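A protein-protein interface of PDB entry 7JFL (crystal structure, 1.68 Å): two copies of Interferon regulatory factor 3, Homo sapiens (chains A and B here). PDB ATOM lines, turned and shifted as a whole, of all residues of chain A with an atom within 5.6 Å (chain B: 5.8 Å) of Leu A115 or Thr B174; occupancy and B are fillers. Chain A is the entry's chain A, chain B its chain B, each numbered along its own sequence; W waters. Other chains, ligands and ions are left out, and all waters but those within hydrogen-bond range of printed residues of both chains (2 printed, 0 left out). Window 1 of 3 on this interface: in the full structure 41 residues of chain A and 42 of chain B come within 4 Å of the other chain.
The side-chain hydroxyl (OG1) of Thr B174 lies close to the side-chain carboxylate (OE1) of Glu A112, 2.3 Å away.
Printed residues of chain B within 4 Å of Glu A112: Thr B174 (2.3 Å).
Printed residues of chain B within 4 Å of Leu A114: Gly B27 (3.5 Å) and Trp B173 (3.98 Å).
Of the printed residues of chain B, Leu A115 touches Pro B172 (3.6 Å) and Thr B174 (3.9 Å).
Of the printed residues of chain A, Gly B27 touches Leu A114 (3.5 Å).
Printed residues of chain A within 4 Å of Pro B172: Leu A115.
Of the printed residues of chain A, Trp B173 touches Leu A114 (3.98 Å).
Of chain A, only Glu A112 (2.3 Å) and Leu A115 (3.9 Å) come within 4 Å of Thr B174.
Hydrophobic or aromatic side chains of chain A that line the printed part of chain B: Leu A114 and Leu A115.
Hydrophobic or aromatic side chains of chain B within 4 Å of the printed part of chain A: Pro B172 and Trp B173.
2 positions are printed for both chains.
Of the 5 pairs that touch across the chains among the printed residues, none has its exchanged pair printed and touching as well.
N of Gly B27 is in hydrogen-bond range of O of Thr B174 (3.3 Å).
The backbone carbonyl oxygen (O) of Glu A112 lies within hydrogen-bond range of the indole nitrogen (NE1) of Trp A160.
OG of Ser A111 sits at hydrogen-bond distance from O of Leu A115, at 2.9 Å.
Among the printed residues, pairs that only touch across the chains: Leu A114 with Gly B27, Leu A114 with Trp B173, Leu A115 with Pro B172 and Leu A115 with Thr B174.
Water W1 lies within hydrogen-bond range of the backbone carbonyl oxygen (O) of Leu A114 (2.7 Å), the indole nitrogen (NE1) of Trp A173 (3.0 Å) and the indole nitrogen (NE1) of Trp B173 (3.0 Å).
Water W2 lies within hydrogen-bond range of O of Gly B27 (2.8 Å), N of Leu A114 (2.8 Å) and N of Glu A113 (3.4 Å).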
ATOM      1  N   SER A 111     -17.505 -25.088 -22.935  1.00  0.00           N
ATOM      2  CA  SER A 111     -18.800 -24.760 -22.361  1.00  0.00           C
ATOM      3  C   SER A 111     -18.623 -23.838 -21.169  1.00  0.00           C
ATOM      4  O   SER A 111     -17.770 -22.950 -21.199  1.00  0.00           O
ATOM      5  CB  SER A 111     -19.552 -26.031 -21.951  1.00  0.00           C
ATOM      6  OG  SER A 111     -20.929 -25.750 -21.725  1.00  0.00           O
ATOM      7  N   GLU A 112     -19.413 -24.044 -20.126  1.00  0.00           N
ATOM      8  CA  GLU A 112     -19.440 -23.138 -18.987  1.00  0.00           C
ATOM      9  C   GLU A 112     -18.789 -23.785 -17.776  1.00  0.00           C
ATOM     10  O   GLU A 112     -18.524 -24.986 -17.754  1.00  0.00           O
ATOM     11  CB  GLU A 112     -20.875 -22.719 -18.678  1.00  0.00           C
ATOM     12  CG  GLU A 112     -21.474 -21.912 -19.817  1.00  0.00           C
ATOM     13  CD  GLU A 112     -22.911 -21.567 -19.577  1.00  0.00           C
ATOM     14  OE1 GLU A 112     -23.543 -22.261 -18.752  1.00  0.00           O
ATOM     15  OE2 GLU A 112     -23.405 -20.606 -20.205  1.00  0.00           O
ATOM     16  N   GLU A 113     -18.553 -22.958 -16.751  1.00  0.00           N
ATOM     17  CA  GLU A 113     -17.811 -23.428 -15.581  1.00  0.00           C
ATOM     18  C   GLU A 113     -18.564 -24.529 -14.841  1.00  0.00           C
ATOM     19  O   GLU A 113     -17.959 -25.515 -14.405  1.00  0.00           O
ATOM     20  CB  GLU A 113     -17.517 -22.259 -14.651  1.00  0.00           C
ATOM     21  CG  GLU A 113     -16.662 -21.164 -15.288  1.00  0.00           C
ATOM     22  CD  GLU A 113     -15.223 -21.162 -14.793  1.00  0.00           C
ATOM     23  OE1 GLU A 113     -14.782 -22.203 -14.269  1.00  0.00           O
ATOM     24  OE2 GLU A 113     -14.538 -20.122 -14.933  1.00  0.00           O
ATOM     25  N   LEU A 114     -19.876 -24.375 -14.667  1.00  0.00           N
ATOM     26  CA  LEU A 114     -20.631 -25.342 -13.881  1.00  0.00           C
ATOM     27  C   LEU A 114     -21.563 -26.200 -14.720  1.00  0.00           C
ATOM     28  O   LEU A 114     -22.374 -26.936 -14.153  1.00  0.00           O
ATOM     29  CB  LEU A 114     -21.427 -24.643 -12.774  1.00  0.00           C
ATOM     30  CG  LEU A 114     -20.670 -23.853 -11.695  1.00  0.00           C
ATOM     31  CD1 LEU A 114     -21.563 -23.624 -10.503  1.00  0.00           C
ATOM     32  CD2 LEU A 114     -19.392 -24.562 -11.273  1.00  0.00           C
ATOM     33  N   LEU A 115     -21.458 -26.149 -16.050  1.00  0.00           N
ATOM     34  CA  LEU A 115     -22.341 -26.944 -16.891  1.00  0.00           C
ATOM     35  C   LEU A 115     -21.586 -27.395 -18.138  1.00  0.00           C
ATOM     36  O   LEU A 115     -21.199 -26.562 -18.962  1.00  0.00           O
ATOM     37  CB  LEU A 115     -23.582 -26.144 -17.282  1.00  0.00           C
ATOM     38  CG  LEU A 115     -24.584 -26.868 -18.172  1.00  0.00           C
ATOM     39  CD1 LEU A 115     -25.102 -28.119 -17.448  1.00  0.00           C
ATOM     40  CD2 LEU A 115     -25.738 -25.918 -18.512  1.00  0.00           C
ATOM     41  N   PRO A 116     -21.343 -28.696 -18.298  1.00  0.00           N
ATOM     42  CA  PRO A 116     -20.619 -29.166 -19.494  1.00  0.00           C
ATOM     43  C   PRO A 116     -21.391 -28.987 -20.786  1.00  0.00           C
ATOM     44  O   PRO A 116     -20.774 -28.823 -21.851  1.00  0.00           O
ATOM     45  CB  PRO A 116     -20.376 -30.654 -19.201  1.00  0.00           C
ATOM     46  CG  PRO A 116     -20.547 -30.801 -17.727  1.00  0.00           C
ATOM     47  CD  PRO A 116     -21.526 -29.755 -17.291  1.00  0.00           C
ATOM     48  N   ASN A 117     -22.720 -29.029 -20.737  1.00  0.00           N
ATOM     49  CA  ASN A 117     -23.519 -28.982 -21.949  1.00  0.00           C
ATOM     50  C   ASN A 117     -23.518 -27.578 -22.536  1.00  0.00           C
ATOM     51  O   ASN A 117     -23.778 -26.598 -21.832  1.00  0.00           O
ATOM     52  CB  ASN A 117     -24.949 -29.428 -21.656  1.00  0.00           C
ATOM     53  CG  ASN A 117     -24.995 -30.805 -21.016  1.00  0.00           C
ATOM     54  OD1 ASN A 117     -24.929 -30.940 -19.788  1.00  0.00           O
ATOM     55  ND2 ASN A 117     -25.069 -31.839 -21.852  1.00  0.00           N
ATOM     56  N   SER A 118     -23.226 -27.484 -23.828  1.00  0.00           N
ATOM     57  CA  SER A 118     -23.409 -26.242 -24.559  1.00  0.00           C
ATOM     58  C   SER A 118     -24.738 -26.187 -25.297  1.00  0.00           C
ATOM     59  O   SER A 118     -25.118 -25.115 -25.783  1.00  0.00           O
ATOM     60  CB  SER A 118     -22.274 -26.053 -25.564  1.00  0.00           C
ATOM     61  OG  SER A 118     -22.268 -27.134 -26.488  1.00  0.00           O
ATOM     62  N   TRP A 160     -14.363 -29.194 -21.431  1.00  0.00           N
ATOM     63  CA  TRP A 160     -14.901 -30.359 -20.761  1.00  0.00           C
ATOM     64  C   TRP A 160     -14.582 -31.592 -21.578  1.00  0.00           C
ATOM     65  O   TRP A 160     -14.726 -31.586 -22.805  1.00  0.00           O
ATOM     66  CB  TRP A 160     -16.401 -30.249 -20.580  1.00  0.00           C
ATOM     67  CG  TRP A 160     -16.817 -29.312 -19.527  1.00  0.00           C
ATOM     68  CD1 TRP A 160     -17.033 -27.976 -19.659  1.00  0.00           C
ATOM     69  CD2 TRP A 160     -17.095 -29.636 -18.166  1.00  0.00           C
ATOM     70  NE1 TRP A 160     -17.439 -27.440 -18.455  1.00  0.00           N
ATOM     71  CE2 TRP A 160     -17.489 -28.444 -17.525  1.00  0.00           C
ATOM     72  CE3 TRP A 160     -17.049 -30.820 -17.423  1.00  0.00           C
ATOM     73  CZ2 TRP A 160     -17.839 -28.401 -16.177  1.00  0.00           C
ATOM     74  CZ3 TRP A 160     -17.414 -30.780 -16.084  1.00  0.00           C
ATOM     75  CH2 TRP A 160     -17.800 -29.571 -15.478  1.00  0.00           C
ATOM     76  N   TRP A 173     -25.596 -34.613 -17.603  1.00  0.00           N
ATOM     77  CA  TRP A 173     -24.165 -34.868 -17.531  1.00  0.00           C
ATOM     78  C   TRP A 173     -23.768 -35.554 -16.237  1.00  0.00           C
ATOM     79  O   TRP A 173     -22.743 -36.244 -16.200  1.00  0.00           O
ATOM     80  CB  TRP A 173     -23.387 -33.557 -17.686  1.00  0.00           C
ATOM     81  CG  TRP A 173     -23.440 -32.622 -16.474  1.00  0.00           C
ATOM     82  CD1 TRP A 173     -24.366 -31.647 -16.219  1.00  0.00           C
ATOM     83  CD2 TRP A 173     -22.497 -32.571 -15.398  1.00  0.00           C
ATOM     84  NE1 TRP A 173     -24.070 -31.012 -15.031  1.00  0.00           N
ATOM     85  CE2 TRP A 173     -22.926 -31.560 -14.511  1.00  0.00           C
ATOM     86  CE3 TRP A 173     -21.338 -33.296 -15.089  1.00  0.00           C
ATOM     87  CZ2 TRP A 173     -22.219 -31.234 -13.349  1.00  0.00           C
ATOM     88  CZ3 TRP A 173     -20.636 -32.977 -13.926  1.00  0.00           C
ATOM     89  CH2 TRP A 173     -21.089 -31.962 -13.066  1.00  0.00           C
ATOM     90  N   TYR B  25     -25.248 -17.439  -8.184  1.00  0.00           N
ATOM     91  CA  TYR B  25     -25.678 -16.335  -9.035  1.00  0.00           C
ATOM     92  C   TYR B  25     -25.085 -16.561 -10.416  1.00  0.00           C
ATOM     93  O   TYR B  25     -23.864 -16.690 -10.549  1.00  0.00           O
ATOM     94  CB  TYR B  25     -25.228 -14.967  -8.520  1.00  0.00           C
ATOM     95  CG  TYR B  25     -25.650 -14.606  -7.127  1.00  0.00           C
ATOM     96  CD1 TYR B  25     -26.772 -15.184  -6.528  1.00  0.00           C
ATOM     97  CD2 TYR B  25     -24.913 -13.671  -6.396  1.00  0.00           C
ATOM     98  CE1 TYR B  25     -27.135 -14.827  -5.220  1.00  0.00           C
ATOM     99  CE2 TYR B  25     -25.276 -13.313  -5.105  1.00  0.00           C
ATOM    100  CZ  TYR B  25     -26.384 -13.896  -4.527  1.00  0.00           C
ATOM    101  OH  TYR B  25     -26.717 -13.512  -3.245  1.00  0.00           O
ATOM    102  N   ARG B  26     -25.943 -16.591 -11.432  1.00  0.00           N
ATOM    103  CA  ARG B  26     -25.504 -16.701 -12.816  1.00  0.00           C
ATOM    104  C   ARG B  26     -24.458 -17.810 -12.975  1.00  0.00           C
ATOM    105  O   ARG B  26     -23.381 -17.627 -13.552  1.00  0.00           O
ATOM    106  CB  ARG B  26     -24.985 -15.340 -13.297  1.00  0.00           C
ATOM    107  CG  ARG B  26     -24.673 -15.246 -14.778  1.00  0.00           C
ATOM    108  CD  ARG B  26     -25.912 -15.055 -15.633  1.00  0.00           C
ATOM    109  NE  ARG B  26     -25.537 -14.643 -16.987  1.00  0.00           N
ATOM    110  CZ  ARG B  26     -26.411 -14.400 -17.958  1.00  0.00           C
ATOM    111  NH1 ARG B  26     -27.710 -14.548 -17.729  1.00  0.00           N
ATOM    112  NH2 ARG B  26     -25.992 -13.994 -19.148  1.00  0.00           N
ATOM    113  N   GLY B  27     -24.773 -18.977 -12.424  1.00  0.00           N
ATOM    114  CA  GLY B  27     -23.921 -20.129 -12.658  1.00  0.00           C
ATOM    115  C   GLY B  27     -22.580 -20.052 -11.968  1.00  0.00           C
ATOM    116  O   GLY B  27     -21.593 -20.600 -12.477  1.00  0.00           O
ATOM    117  N   LEU B 115     -26.909 -30.379 -10.459  1.00  0.00           N
ATOM    118  CA  LEU B 115     -27.739 -30.012 -11.601  1.00  0.00           C
ATOM    119  C   LEU B 115     -29.175 -29.781 -11.148  1.00  0.00           C
ATOM    120  O   LEU B 115     -29.818 -30.709 -10.648  1.00  0.00           O
ATOM    121  CB  LEU B 115     -27.701 -31.104 -12.679  1.00  0.00           C
ATOM    122  CG  LEU B 115     -28.491 -30.855 -13.959  1.00  0.00           C
ATOM    123  CD1 LEU B 115     -27.926 -29.641 -14.714  1.00  0.00           C
ATOM    124  CD2 LEU B 115     -28.452 -32.095 -14.844  1.00  0.00           C
ATOM    125  N   PRO B 172     -30.127 -23.005 -20.237  1.00  0.00           N
ATOM    126  CA  PRO B 172     -29.243 -23.551 -19.196  1.00  0.00           C
ATOM    127  C   PRO B 172     -29.469 -22.857 -17.866  1.00  0.00           C
ATOM    128  O   PRO B 172     -29.665 -21.642 -17.799  1.00  0.00           O
ATOM    129  CB  PRO B 172     -27.833 -23.278 -19.744  1.00  0.00           C
ATOM    130  CG  PRO B 172     -28.012 -22.236 -20.771  1.00  0.00           C
ATOM    131  CD  PRO B 172     -29.371 -22.426 -21.355  1.00  0.00           C
ATOM    132  N   TRP B 173     -29.436 -23.646 -16.786  1.00  0.00           N
ATOM    133  CA  TRP B 173     -29.702 -23.097 -15.464  1.00  0.00           C
ATOM    134  C   TRP B 173     -28.669 -22.062 -15.045  1.00  0.00           C
ATOM    135  O   TRP B 173     -28.952 -21.230 -14.172  1.00  0.00           O
ATOM    136  CB  TRP B 173     -29.752 -24.224 -14.440  1.00  0.00           C
ATOM    137  CG  TRP B 173     -28.410 -24.821 -14.105  1.00  0.00           C
ATOM    138  CD1 TRP B 173     -27.803 -25.881 -14.719  1.00  0.00           C
ATOM    139  CD2 TRP B 173     -27.537 -24.417 -13.043  1.00  0.00           C
ATOM    140  NE1 TRP B 173     -26.598 -26.151 -14.107  1.00  0.00           N
ATOM    141  CE2 TRP B 173     -26.410 -25.261 -13.084  1.00  0.00           C
ATOM    142  CE3 TRP B 173     -27.594 -23.408 -12.074  1.00  0.00           C
ATOM    143  CZ2 TRP B 173     -25.352 -25.143 -12.173  1.00  0.00           C
ATOM    144  CZ3 TRP B 173     -26.543 -23.297 -11.165  1.00  0.00           C
ATOM    145  CH2 TRP B 173     -25.435 -24.156 -11.233  1.00  0.00           C
ATOM    146  N   THR B 174     -27.476 -22.098 -15.643  1.00  0.00           N
ATOM    147  CA  THR B 174     -26.423 -21.138 -15.331  1.00  0.00           C
ATOM    148  C   THR B 174     -26.754 -19.731 -15.810  1.00  0.00           C
ATOM    149  O   THR B 174     -26.032 -18.792 -15.462  1.00  0.00           O
ATOM    150  CB  THR B 174     -25.110 -21.597 -15.963  1.00  0.00           C
ATOM    151  OG1 THR B 174     -25.331 -21.851 -17.349  1.00  0.00           O
ATOM    152  CG2 THR B 174     -24.632 -22.882 -15.318  1.00  0.00           C
ATOM    153  N   LYS B 175     -27.813 -19.568 -16.603  1.00  0.00           N
ATOM    154  CA  LYS B 175     -28.238 -18.236 -17.014  1.00  0.00           C
ATOM    155  C   LYS B 175     -29.042 -17.539 -15.928  1.00  0.00           C
ATOM    156  O   LYS B 175     -29.152 -16.308 -15.948  1.00  0.00           O
ATOM    157  CB  LYS B 175     -29.090 -18.311 -18.286  1.00  0.00           C
ATOM    158  CG  LYS B 175     -28.341 -18.726 -19.526  1.00  0.00           C
ATOM    159  CD  LYS B 175     -27.434 -17.623 -20.008  1.00  0.00           C
ATOM    160  CE  LYS B 175     -27.003 -17.859 -21.452  1.00  0.00           C
ATOM    161  NZ  LYS B 175     -26.227 -16.698 -21.962  1.00  0.00           N
ATOM    162  N   ARG B 176     -29.610 -18.299 -15.001  1.00  0.00           N
ATOM    163  CA  ARG B 176     -30.549 -17.730 -14.040  1.00  0.00           C
ATOM    164  C   ARG B 176     -29.820 -16.874 -13.014  1.00  0.00           C
ATOM    165  O   ARG B 176     -28.705 -17.191 -12.594  1.00  0.00           O
ATOM    166  CB  ARG B 176     -31.333 -18.843 -13.350  1.00  0.00           C
ATOM    167  CG  ARG B 176     -32.449 -19.414 -14.226  1.00  0.00           C
ATOM    168  CD  ARG B 176     -33.482 -18.348 -14.535  1.00  0.00           C
ATOM    169  NE  ARG B 176     -34.574 -18.850 -15.357  1.00  0.00           N
ATOM    170  CZ  ARG B 176     -34.625 -18.774 -16.680  1.00  0.00           C
ATOM    171  NH1 ARG B 176     -33.627 -18.223 -17.369  1.00  0.00           N
ATOM    172  NH2 ARG B 176     -35.685 -19.256 -17.322  1.00  0.00           N
HETATM  173  O   HOH W   1     -24.634 -28.397 -13.762  1.00  0.00           O
HETATM  174  O   HOH W   2     -21.233 -21.934 -14.884  1.00  0.00           O
